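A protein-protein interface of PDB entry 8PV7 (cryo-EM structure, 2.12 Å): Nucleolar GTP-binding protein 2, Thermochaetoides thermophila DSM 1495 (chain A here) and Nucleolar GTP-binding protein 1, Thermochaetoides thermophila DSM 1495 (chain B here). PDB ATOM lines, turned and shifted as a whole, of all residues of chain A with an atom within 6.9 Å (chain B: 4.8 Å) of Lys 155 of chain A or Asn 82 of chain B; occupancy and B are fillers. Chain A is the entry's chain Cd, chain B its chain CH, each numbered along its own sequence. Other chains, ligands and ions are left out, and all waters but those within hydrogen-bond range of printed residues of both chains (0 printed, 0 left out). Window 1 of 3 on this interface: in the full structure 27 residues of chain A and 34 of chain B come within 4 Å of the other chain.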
ATOM      1  N   THR A 135      28.370 -20.642  24.865  1.00  0.00           N
ATOM      2  CA  THR A 135      28.611 -21.294  23.581  1.00  0.00           C
ATOM      3  C   THR A 135      29.813 -22.226  23.651  1.00  0.00           C
ATOM      4  O   THR A 135      29.805 -23.298  23.042  1.00  0.00           O
ATOM      5  CB  THR A 135      28.799 -20.260  22.467  1.00  0.00           C
ATOM      6  OG1 THR A 135      29.814 -19.323  22.832  1.00  0.00           O
ATOM      7  CG2 THR A 135      27.508 -19.522  22.198  1.00  0.00           C
ATOM      8  N   ARG A 138      28.729 -25.337  25.596  1.00  0.00           N
ATOM      9  CA  ARG A 138      27.884 -26.185  24.765  1.00  0.00           C
ATOM     10  C   ARG A 138      28.691 -26.897  23.684  1.00  0.00           C
ATOM     11  O   ARG A 138      28.523 -28.101  23.473  1.00  0.00           O
ATOM     12  CB  ARG A 138      26.772 -25.351  24.138  1.00  0.00           C
ATOM     13  CG  ARG A 138      25.776 -26.142  23.331  1.00  0.00           C
ATOM     14  CD  ARG A 138      24.931 -25.250  22.435  1.00  0.00           C
ATOM     15  NE  ARG A 138      24.481 -24.039  23.109  1.00  0.00           N
ATOM     16  CZ  ARG A 138      24.888 -22.811  22.813  1.00  0.00           C
ATOM     17  NH1 ARG A 138      25.747 -22.585  21.835  1.00  0.00           N
ATOM     18  NH2 ARG A 138      24.423 -21.788  23.522  1.00  0.00           N
ATOM     19  N   GLU A 139      29.544 -26.170  22.967  1.00  0.00           N
ATOM     20  CA  GLU A 139      30.334 -26.727  21.870  1.00  0.00           C
ATOM     21  C   GLU A 139      31.787 -26.311  22.054  1.00  0.00           C
ATOM     22  O   GLU A 139      32.143 -25.160  21.745  1.00  0.00           O
ATOM     23  CB  GLU A 139      29.813 -26.261  20.515  1.00  0.00           C
ATOM     24  CG  GLU A 139      28.304 -26.292  20.355  1.00  0.00           C
ATOM     25  CD  GLU A 139      27.707 -24.921  20.102  1.00  0.00           C
ATOM     26  OE1 GLU A 139      26.753 -24.822  19.306  1.00  0.00           O
ATOM     27  OE2 GLU A 139      28.195 -23.938  20.695  1.00  0.00           O
ATOM     28  N   ARG A 151      31.367 -31.437  14.377  1.00  0.00           N
ATOM     29  CA  ARG A 151      30.290 -30.553  13.964  1.00  0.00           C
ATOM     30  C   ARG A 151      29.850 -30.870  12.540  1.00  0.00           C
ATOM     31  O   ARG A 151      30.656 -30.869  11.609  1.00  0.00           O
ATOM     32  CB  ARG A 151      30.744 -29.099  14.072  1.00  0.00           C
ATOM     33  CG  ARG A 151      29.878 -28.094  13.343  1.00  0.00           C
ATOM     34  CD  ARG A 151      30.389 -26.683  13.575  1.00  0.00           C
ATOM     35  NE  ARG A 151      29.644 -25.679  12.824  1.00  0.00           N
ATOM     36  CZ  ARG A 151      30.057 -25.132  11.690  1.00  0.00           C
ATOM     37  NH1 ARG A 151      31.201 -25.482  11.132  1.00  0.00           N
ATOM     38  NH2 ARG A 151      29.299 -24.217  11.099  1.00  0.00           N
ATOM     39  N   ARG A 153      26.123 -29.964  11.543  1.00  0.00           N
ATOM     40  CA  ARG A 153      25.058 -29.014  11.248  1.00  0.00           C
ATOM     41  C   ARG A 153      25.502 -27.600  11.578  1.00  0.00           C
ATOM     42  O   ARG A 153      25.889 -27.333  12.721  1.00  0.00           O
ATOM     43  CB  ARG A 153      23.803 -29.354  12.043  1.00  0.00           C
ATOM     44  CG  ARG A 153      23.145 -30.662  11.661  1.00  0.00           C
ATOM     45  CD  ARG A 153      22.631 -30.635  10.241  1.00  0.00           C
ATOM     46  NE  ARG A 153      22.059 -31.915   9.846  1.00  0.00           N
ATOM     47  CZ  ARG A 153      22.761 -32.939   9.379  1.00  0.00           C
ATOM     48  NH1 ARG A 153      24.071 -32.867   9.227  1.00  0.00           N
ATOM     49  NH2 ARG A 153      22.128 -34.061   9.047  1.00  0.00           N
ATOM     50  N   PRO A 154      25.462 -26.673  10.629  1.00  0.00           N
ATOM     51  CA  PRO A 154      25.796 -25.279  10.931  1.00  0.00           C
ATOM     52  C   PRO A 154      24.662 -24.575  11.667  1.00  0.00           C
ATOM     53  O   PRO A 154      23.536 -25.059  11.757  1.00  0.00           O
ATOM     54  CB  PRO A 154      26.017 -24.668   9.545  1.00  0.00           C
ATOM     55  CG  PRO A 154      25.146 -25.477   8.652  1.00  0.00           C
ATOM     56  CD  PRO A 154      25.151 -26.875   9.204  1.00  0.00           C
ATOM     57  N   LYS A 155      24.985 -23.402  12.199  1.00  0.00           N
ATOM     58  CA  LYS A 155      24.002 -22.531  12.829  1.00  0.00           C
ATOM     59  C   LYS A 155      23.610 -21.443  11.836  1.00  0.00           C
ATOM     60  O   LYS A 155      24.468 -20.695  11.360  1.00  0.00           O
ATOM     61  CB  LYS A 155      24.557 -21.924  14.116  1.00  0.00           C
ATOM     62  CG  LYS A 155      23.602 -20.980  14.811  1.00  0.00           C
ATOM     63  CD  LYS A 155      24.285 -20.248  15.946  1.00  0.00           C
ATOM     64  CE  LYS A 155      23.376 -19.195  16.547  1.00  0.00           C
ATOM     65  NZ  LYS A 155      24.087 -18.362  17.553  1.00  0.00           N
ATOM     66  N   LEU A 156      22.324 -21.366  11.516  1.00  0.00           N
ATOM     67  CA  LEU A 156      21.825 -20.474  10.483  1.00  0.00           C
ATOM     68  C   LEU A 156      20.862 -19.449  11.068  1.00  0.00           C
ATOM     69  O   LEU A 156      20.213 -19.680  12.090  1.00  0.00           O
ATOM     70  CB  LEU A 156      21.133 -21.268   9.367  1.00  0.00           C
ATOM     71  CG  LEU A 156      21.956 -22.401   8.746  1.00  0.00           C
ATOM     72  CD1 LEU A 156      21.126 -23.202   7.761  1.00  0.00           C
ATOM     73  CD2 LEU A 156      23.212 -21.867   8.075  1.00  0.00           C
ATOM     74  N   SER A 157      20.784 -18.300  10.402  1.00  0.00           N
ATOM     75  CA  SER A 157      19.843 -17.243  10.746  1.00  0.00           C
ATOM     76  C   SER A 157      18.537 -17.357   9.975  1.00  0.00           C
ATOM     77  O   SER A 157      17.679 -16.479  10.092  1.00  0.00           O
ATOM     78  CB  SER A 157      20.471 -15.873  10.496  1.00  0.00           C
ATOM     79  OG  SER A 157      21.622 -15.682  11.293  1.00  0.00           O
ATOM     80  N   PHE A 158      18.373 -18.413   9.190  1.00  0.00           N
ATOM     81  CA  PHE A 158      17.210 -18.595   8.342  1.00  0.00           C
ATOM     82  C   PHE A 158      16.776 -20.047   8.439  1.00  0.00           C
ATOM     83  O   PHE A 158      17.546 -20.918   8.846  1.00  0.00           O
ATOM     84  CB  PHE A 158      17.512 -18.202   6.885  1.00  0.00           C
ATOM     85  CG  PHE A 158      18.843 -18.688   6.388  1.00  0.00           C
ATOM     86  CD1 PHE A 158      18.966 -19.939   5.814  1.00  0.00           C
ATOM     87  CD2 PHE A 158      19.975 -17.895   6.500  1.00  0.00           C
ATOM     88  CE1 PHE A 158      20.184 -20.392   5.365  1.00  0.00           C
ATOM     89  CE2 PHE A 158      21.195 -18.348   6.056  1.00  0.00           C
ATOM     90  CZ  PHE A 158      21.299 -19.600   5.490  1.00  0.00           C
ATOM     91  N   ARG B  78      31.371 -13.955   4.253  1.00  0.00           N
ATOM     92  CA  ARG B  78      30.896 -14.009   5.632  1.00  0.00           C
ATOM     93  C   ARG B  78      30.096 -15.280   5.896  1.00  0.00           C
ATOM     94  O   ARG B  78      30.349 -15.993   6.879  1.00  0.00           O
ATOM     95  CB  ARG B  78      30.054 -12.766   5.927  1.00  0.00           C
ATOM     96  CG  ARG B  78      29.632 -12.588   7.372  1.00  0.00           C
ATOM     97  CD  ARG B  78      28.874 -11.284   7.552  1.00  0.00           C
ATOM     98  NE  ARG B  78      28.721 -10.916   8.956  1.00  0.00           N
ATOM     99  CZ  ARG B  78      28.189  -9.778   9.381  1.00  0.00           C
ATOM    100  NH1 ARG B  78      27.749  -8.861   8.534  1.00  0.00           N
ATOM    101  NH2 ARG B  78      28.101  -9.549  10.687  1.00  0.00           N
ATOM    102  N   ASP B  79      29.157 -15.607   5.003  1.00  0.00           N
ATOM    103  CA  ASP B  79      28.355 -16.808   5.192  1.00  0.00           C
ATOM    104  C   ASP B  79      29.184 -18.072   5.012  1.00  0.00           C
ATOM    105  O   ASP B  79      29.000 -19.039   5.754  1.00  0.00           O
ATOM    106  CB  ASP B  79      27.161 -16.802   4.244  1.00  0.00           C
ATOM    107  CG  ASP B  79      25.988 -16.041   4.810  1.00  0.00           C
ATOM    108  OD1 ASP B  79      26.192 -14.902   5.277  1.00  0.00           O
ATOM    109  OD2 ASP B  79      24.867 -16.584   4.813  1.00  0.00           O
ATOM    110  N   LEU B  80      30.113 -18.074   4.053  1.00  0.00           N
ATOM    111  CA  LEU B  80      30.977 -19.230   3.855  1.00  0.00           C
ATOM    112  C   LEU B  80      31.873 -19.455   5.062  1.00  0.00           C
ATOM    113  O   LEU B  80      32.098 -20.596   5.474  1.00  0.00           O
ATOM    114  CB  LEU B  80      31.823 -19.053   2.595  1.00  0.00           C
ATOM    115  CG  LEU B  80      32.750 -20.227   2.280  1.00  0.00           C
ATOM    116  CD1 LEU B  80      31.958 -21.505   2.060  1.00  0.00           C
ATOM    117  CD2 LEU B  80      33.643 -19.925   1.093  1.00  0.00           C
ATOM    118  N   MET B  81      32.404 -18.373   5.629  1.00  0.00           N
ATOM    119  CA  MET B  81      33.248 -18.497   6.804  1.00  0.00           C
ATOM    120  C   MET B  81      32.457 -19.045   7.975  1.00  0.00           C
ATOM    121  O   MET B  81      32.970 -19.877   8.719  1.00  0.00           O
ATOM    122  CB  MET B  81      33.865 -17.151   7.159  1.00  0.00           C
ATOM    123  CG  MET B  81      35.326 -17.046   6.804  1.00  0.00           C
ATOM    124  SD  MET B  81      35.750 -15.343   6.430  1.00  0.00           S
ATOM    125  CE  MET B  81      37.035 -15.548   5.205  1.00  0.00           C
ATOM    126  N   ASN B  82      31.197 -18.609   8.132  1.00  0.00           N
ATOM    127  CA  ASN B  82      30.324 -19.196   9.148  1.00  0.00           C
ATOM    128  C   ASN B  82      30.064 -20.681   8.885  1.00  0.00           C
ATOM    129  O   ASN B  82      29.953 -21.473   9.826  1.00  0.00           O
ATOM    130  CB  ASN B  82      28.999 -18.435   9.220  1.00  0.00           C
ATOM    131  CG  ASN B  82      27.961 -19.143  10.078  1.00  0.00           C
ATOM    132  OD1 ASN B  82      28.111 -19.241  11.291  1.00  0.00           O
ATOM    133  ND2 ASN B  82      26.923 -19.664   9.446  1.00  0.00           N
ATOM    134  N   ILE B  83      29.937 -21.074   7.616  1.00  0.00           N
ATOM    135  CA  ILE B  83      29.711 -22.486   7.303  1.00  0.00           C
ATOM    136  C   ILE B  83      30.942 -23.321   7.651  1.00  0.00           C
ATOM    137  O   ILE B  83      30.832 -24.392   8.254  1.00  0.00           O
ATOM    138  CB  ILE B  83      29.303 -22.659   5.824  1.00  0.00           C
ATOM    139  CG1 ILE B  83      27.932 -22.041   5.546  1.00  0.00           C
ATOM    140  CG2 ILE B  83      29.307 -24.121   5.418  1.00  0.00           C
ATOM    141  CD1 ILE B  83      26.794 -22.690   6.256  1.00  0.00           C
ATOM    142  N   LEU B  84      32.131 -22.842   7.285  1.00  0.00           N
ATOM    143  CA  LEU B  84      33.349 -23.633   7.470  1.00  0.00           C
ATOM    144  C   LEU B  84      33.763 -23.701   8.932  1.00  0.00           C
ATOM    145  O   LEU B  84      34.123 -24.768   9.436  1.00  0.00           O
ATOM    146  CB  LEU B  84      34.486 -23.050   6.639  1.00  0.00           C
ATOM    147  CG  LEU B  84      34.270 -23.024   5.132  1.00  0.00           C
ATOM    148  CD1 LEU B  84      35.371 -22.231   4.473  1.00  0.00           C
ATOM    149  CD2 LEU B  84      34.207 -24.433   4.602  1.00  0.00           C
ATOM    150  N   TYR B  85      33.744 -22.568   9.618  1.00  0.00           N
ATOM    151  CA  TYR B  85      34.054 -22.480  11.035  1.00  0.00           C
ATOM    152  C   TYR B  85      32.878 -21.773  11.676  1.00  0.00           C
ATOM    153  O   TYR B  85      32.341 -20.842  11.085  1.00  0.00           O
ATOM    154  CB  TYR B  85      35.354 -21.703  11.258  1.00  0.00           C
ATOM    155  CG  TYR B  85      36.198 -21.569  10.010  1.00  0.00           C
ATOM    156  CD1 TYR B  85      37.059 -22.589   9.619  1.00  0.00           C
ATOM    157  CD2 TYR B  85      36.122 -20.437   9.209  1.00  0.00           C
ATOM    158  CE1 TYR B  85      37.821 -22.479   8.484  1.00  0.00           C
ATOM    159  CE2 TYR B  85      36.881 -20.321   8.063  1.00  0.00           C
ATOM    160  CZ  TYR B  85      37.732 -21.346   7.706  1.00  0.00           C
ATOM    161  OH  TYR B  85      38.501 -21.251   6.570  1.00  0.00           O
ATOM    162  N   ASP B  86      32.445 -22.213  12.847  1.00  0.00           N
ATOM    163  CA  ASP B  86      31.297 -21.552  13.453  1.00  0.00           C
ATOM    164  C   ASP B  86      31.645 -20.097  13.763  1.00  0.00           C
ATOM    165  O   ASP B  86      32.699 -19.808  14.332  1.00  0.00           O
ATOM    166  CB  ASP B  86      30.856 -22.290  14.712  1.00  0.00           C
ATOM    167  CG  ASP B  86      29.831 -21.521  15.504  1.00  0.00           C
ATOM    168  OD1 ASP B  86      28.768 -21.193  14.944  1.00  0.00           O
ATOM    169  OD2 ASP B  86      30.086 -21.244  16.690  1.00  0.00           O
ATOM    170  N   ALA B  87      30.789 -19.180  13.300  1.00  0.00           N
ATOM    171  CA  ALA B  87      31.092 -17.752  13.385  1.00  0.00           C
ATOM    172  C   ALA B  87      31.155 -17.278  14.829  1.00  0.00           C
ATOM    173  O   ALA B  87      31.973 -16.413  15.170  1.00  0.00           O
ATOM    174  CB  ALA B  87      30.055 -16.946  12.608  1.00  0.00           C
ATOM    175  N   ASP B  88      30.296 -17.838  15.686  1.00  0.00           N
ATOM    176  CA  ASP B  88      30.374 -17.568  17.115  1.00  0.00           C
ATOM    177  C   ASP B  88      31.717 -17.997  17.681  1.00  0.00           C
ATOM    178  O   ASP B  88      32.343 -17.241  18.420  1.00  0.00           O
ATOM    179  CB  ASP B  88      29.243 -18.277  17.854  1.00  0.00           C
ATOM    180  CG  ASP B  88      27.893 -17.659  17.591  1.00  0.00           C
ATOM    181  OD1 ASP B  88      27.828 -16.444  17.317  1.00  0.00           O
ATOM    182  OD2 ASP B  88      26.888 -18.389  17.650  1.00  0.00           O
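NH2 of Arg 151 of chain A is in hydrogen-bond range of O of Asn 82 of chain B.
NH1 of Arg 151 of chain A is in hydrogen-bond range of O of Ile 83 of chain B (3.1 Å).
The backbone carbonyl oxygen (O) of Leu 84 of chain B is in hydrogen-bond range of the guanidinium group (NH1) of Arg 151 of chain A, at 3.5 Å.
The side-chain amide nitrogen (ND2) of Asn 82 of chain B is in hydrogen-bond range of the backbone carbonyl oxygen (O) of Lys 155 of chain A.
The side-chain amino group (NZ) of Lys 155 of chain A is in salt-bridge range of the side-chain carboxylate (OD2) of Asp 88 of chain B, 2.8 Å away.
OD1 of Asn 82 of chain B sits close to N of Ala 87 of chain B.
Hydrophobic or aromatic side chains of chain A that line the printed part of chain B: Pro 154.
Hydrophobic or aromatic side chains of chain B within 4 Å of the printed part of chain A: Ile 83.
Among the printed residues, 7 pairs touch across the chains.
NH1 of Arg 151 of chain A touches N of Asp 86 of chain B (3.9 Å).
Pro 154 of chain A touches Ile 83 of chain B.
Lys 155 of chain A touches just these residues of chain B: Asn 82 and Asp 88.
Of chain A, only Arg 151 (3.1 Å) and Lys 155 (3.3 Å) come within 4 Å of Asn 82 of chain B.
Of the printed residues of chain B, Arg 151 of chain A touches Asn 82 (3.1 Å), Ile 83 (3.1 Å), Leu 84 (3.5 Å) and Asp 86 (3.9 Å).
Printed residues of chain B within 4 Å of Pro 154 of chain A: Ile 83 (3.9 Å).
Of the printed residues of chain A, Ile 83 of chain B touches Arg 151 (3.1 Å) and Pro 154 (3.9 Å).
The nearest residue of chain B that does not touch Lys 155 of chain A is Asp 86 of chain B (4.4 Å).
The nearest printed residue of chain B that does not touch Arg 151 of chain A is Tyr 85 of chain B (4.1 Å).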
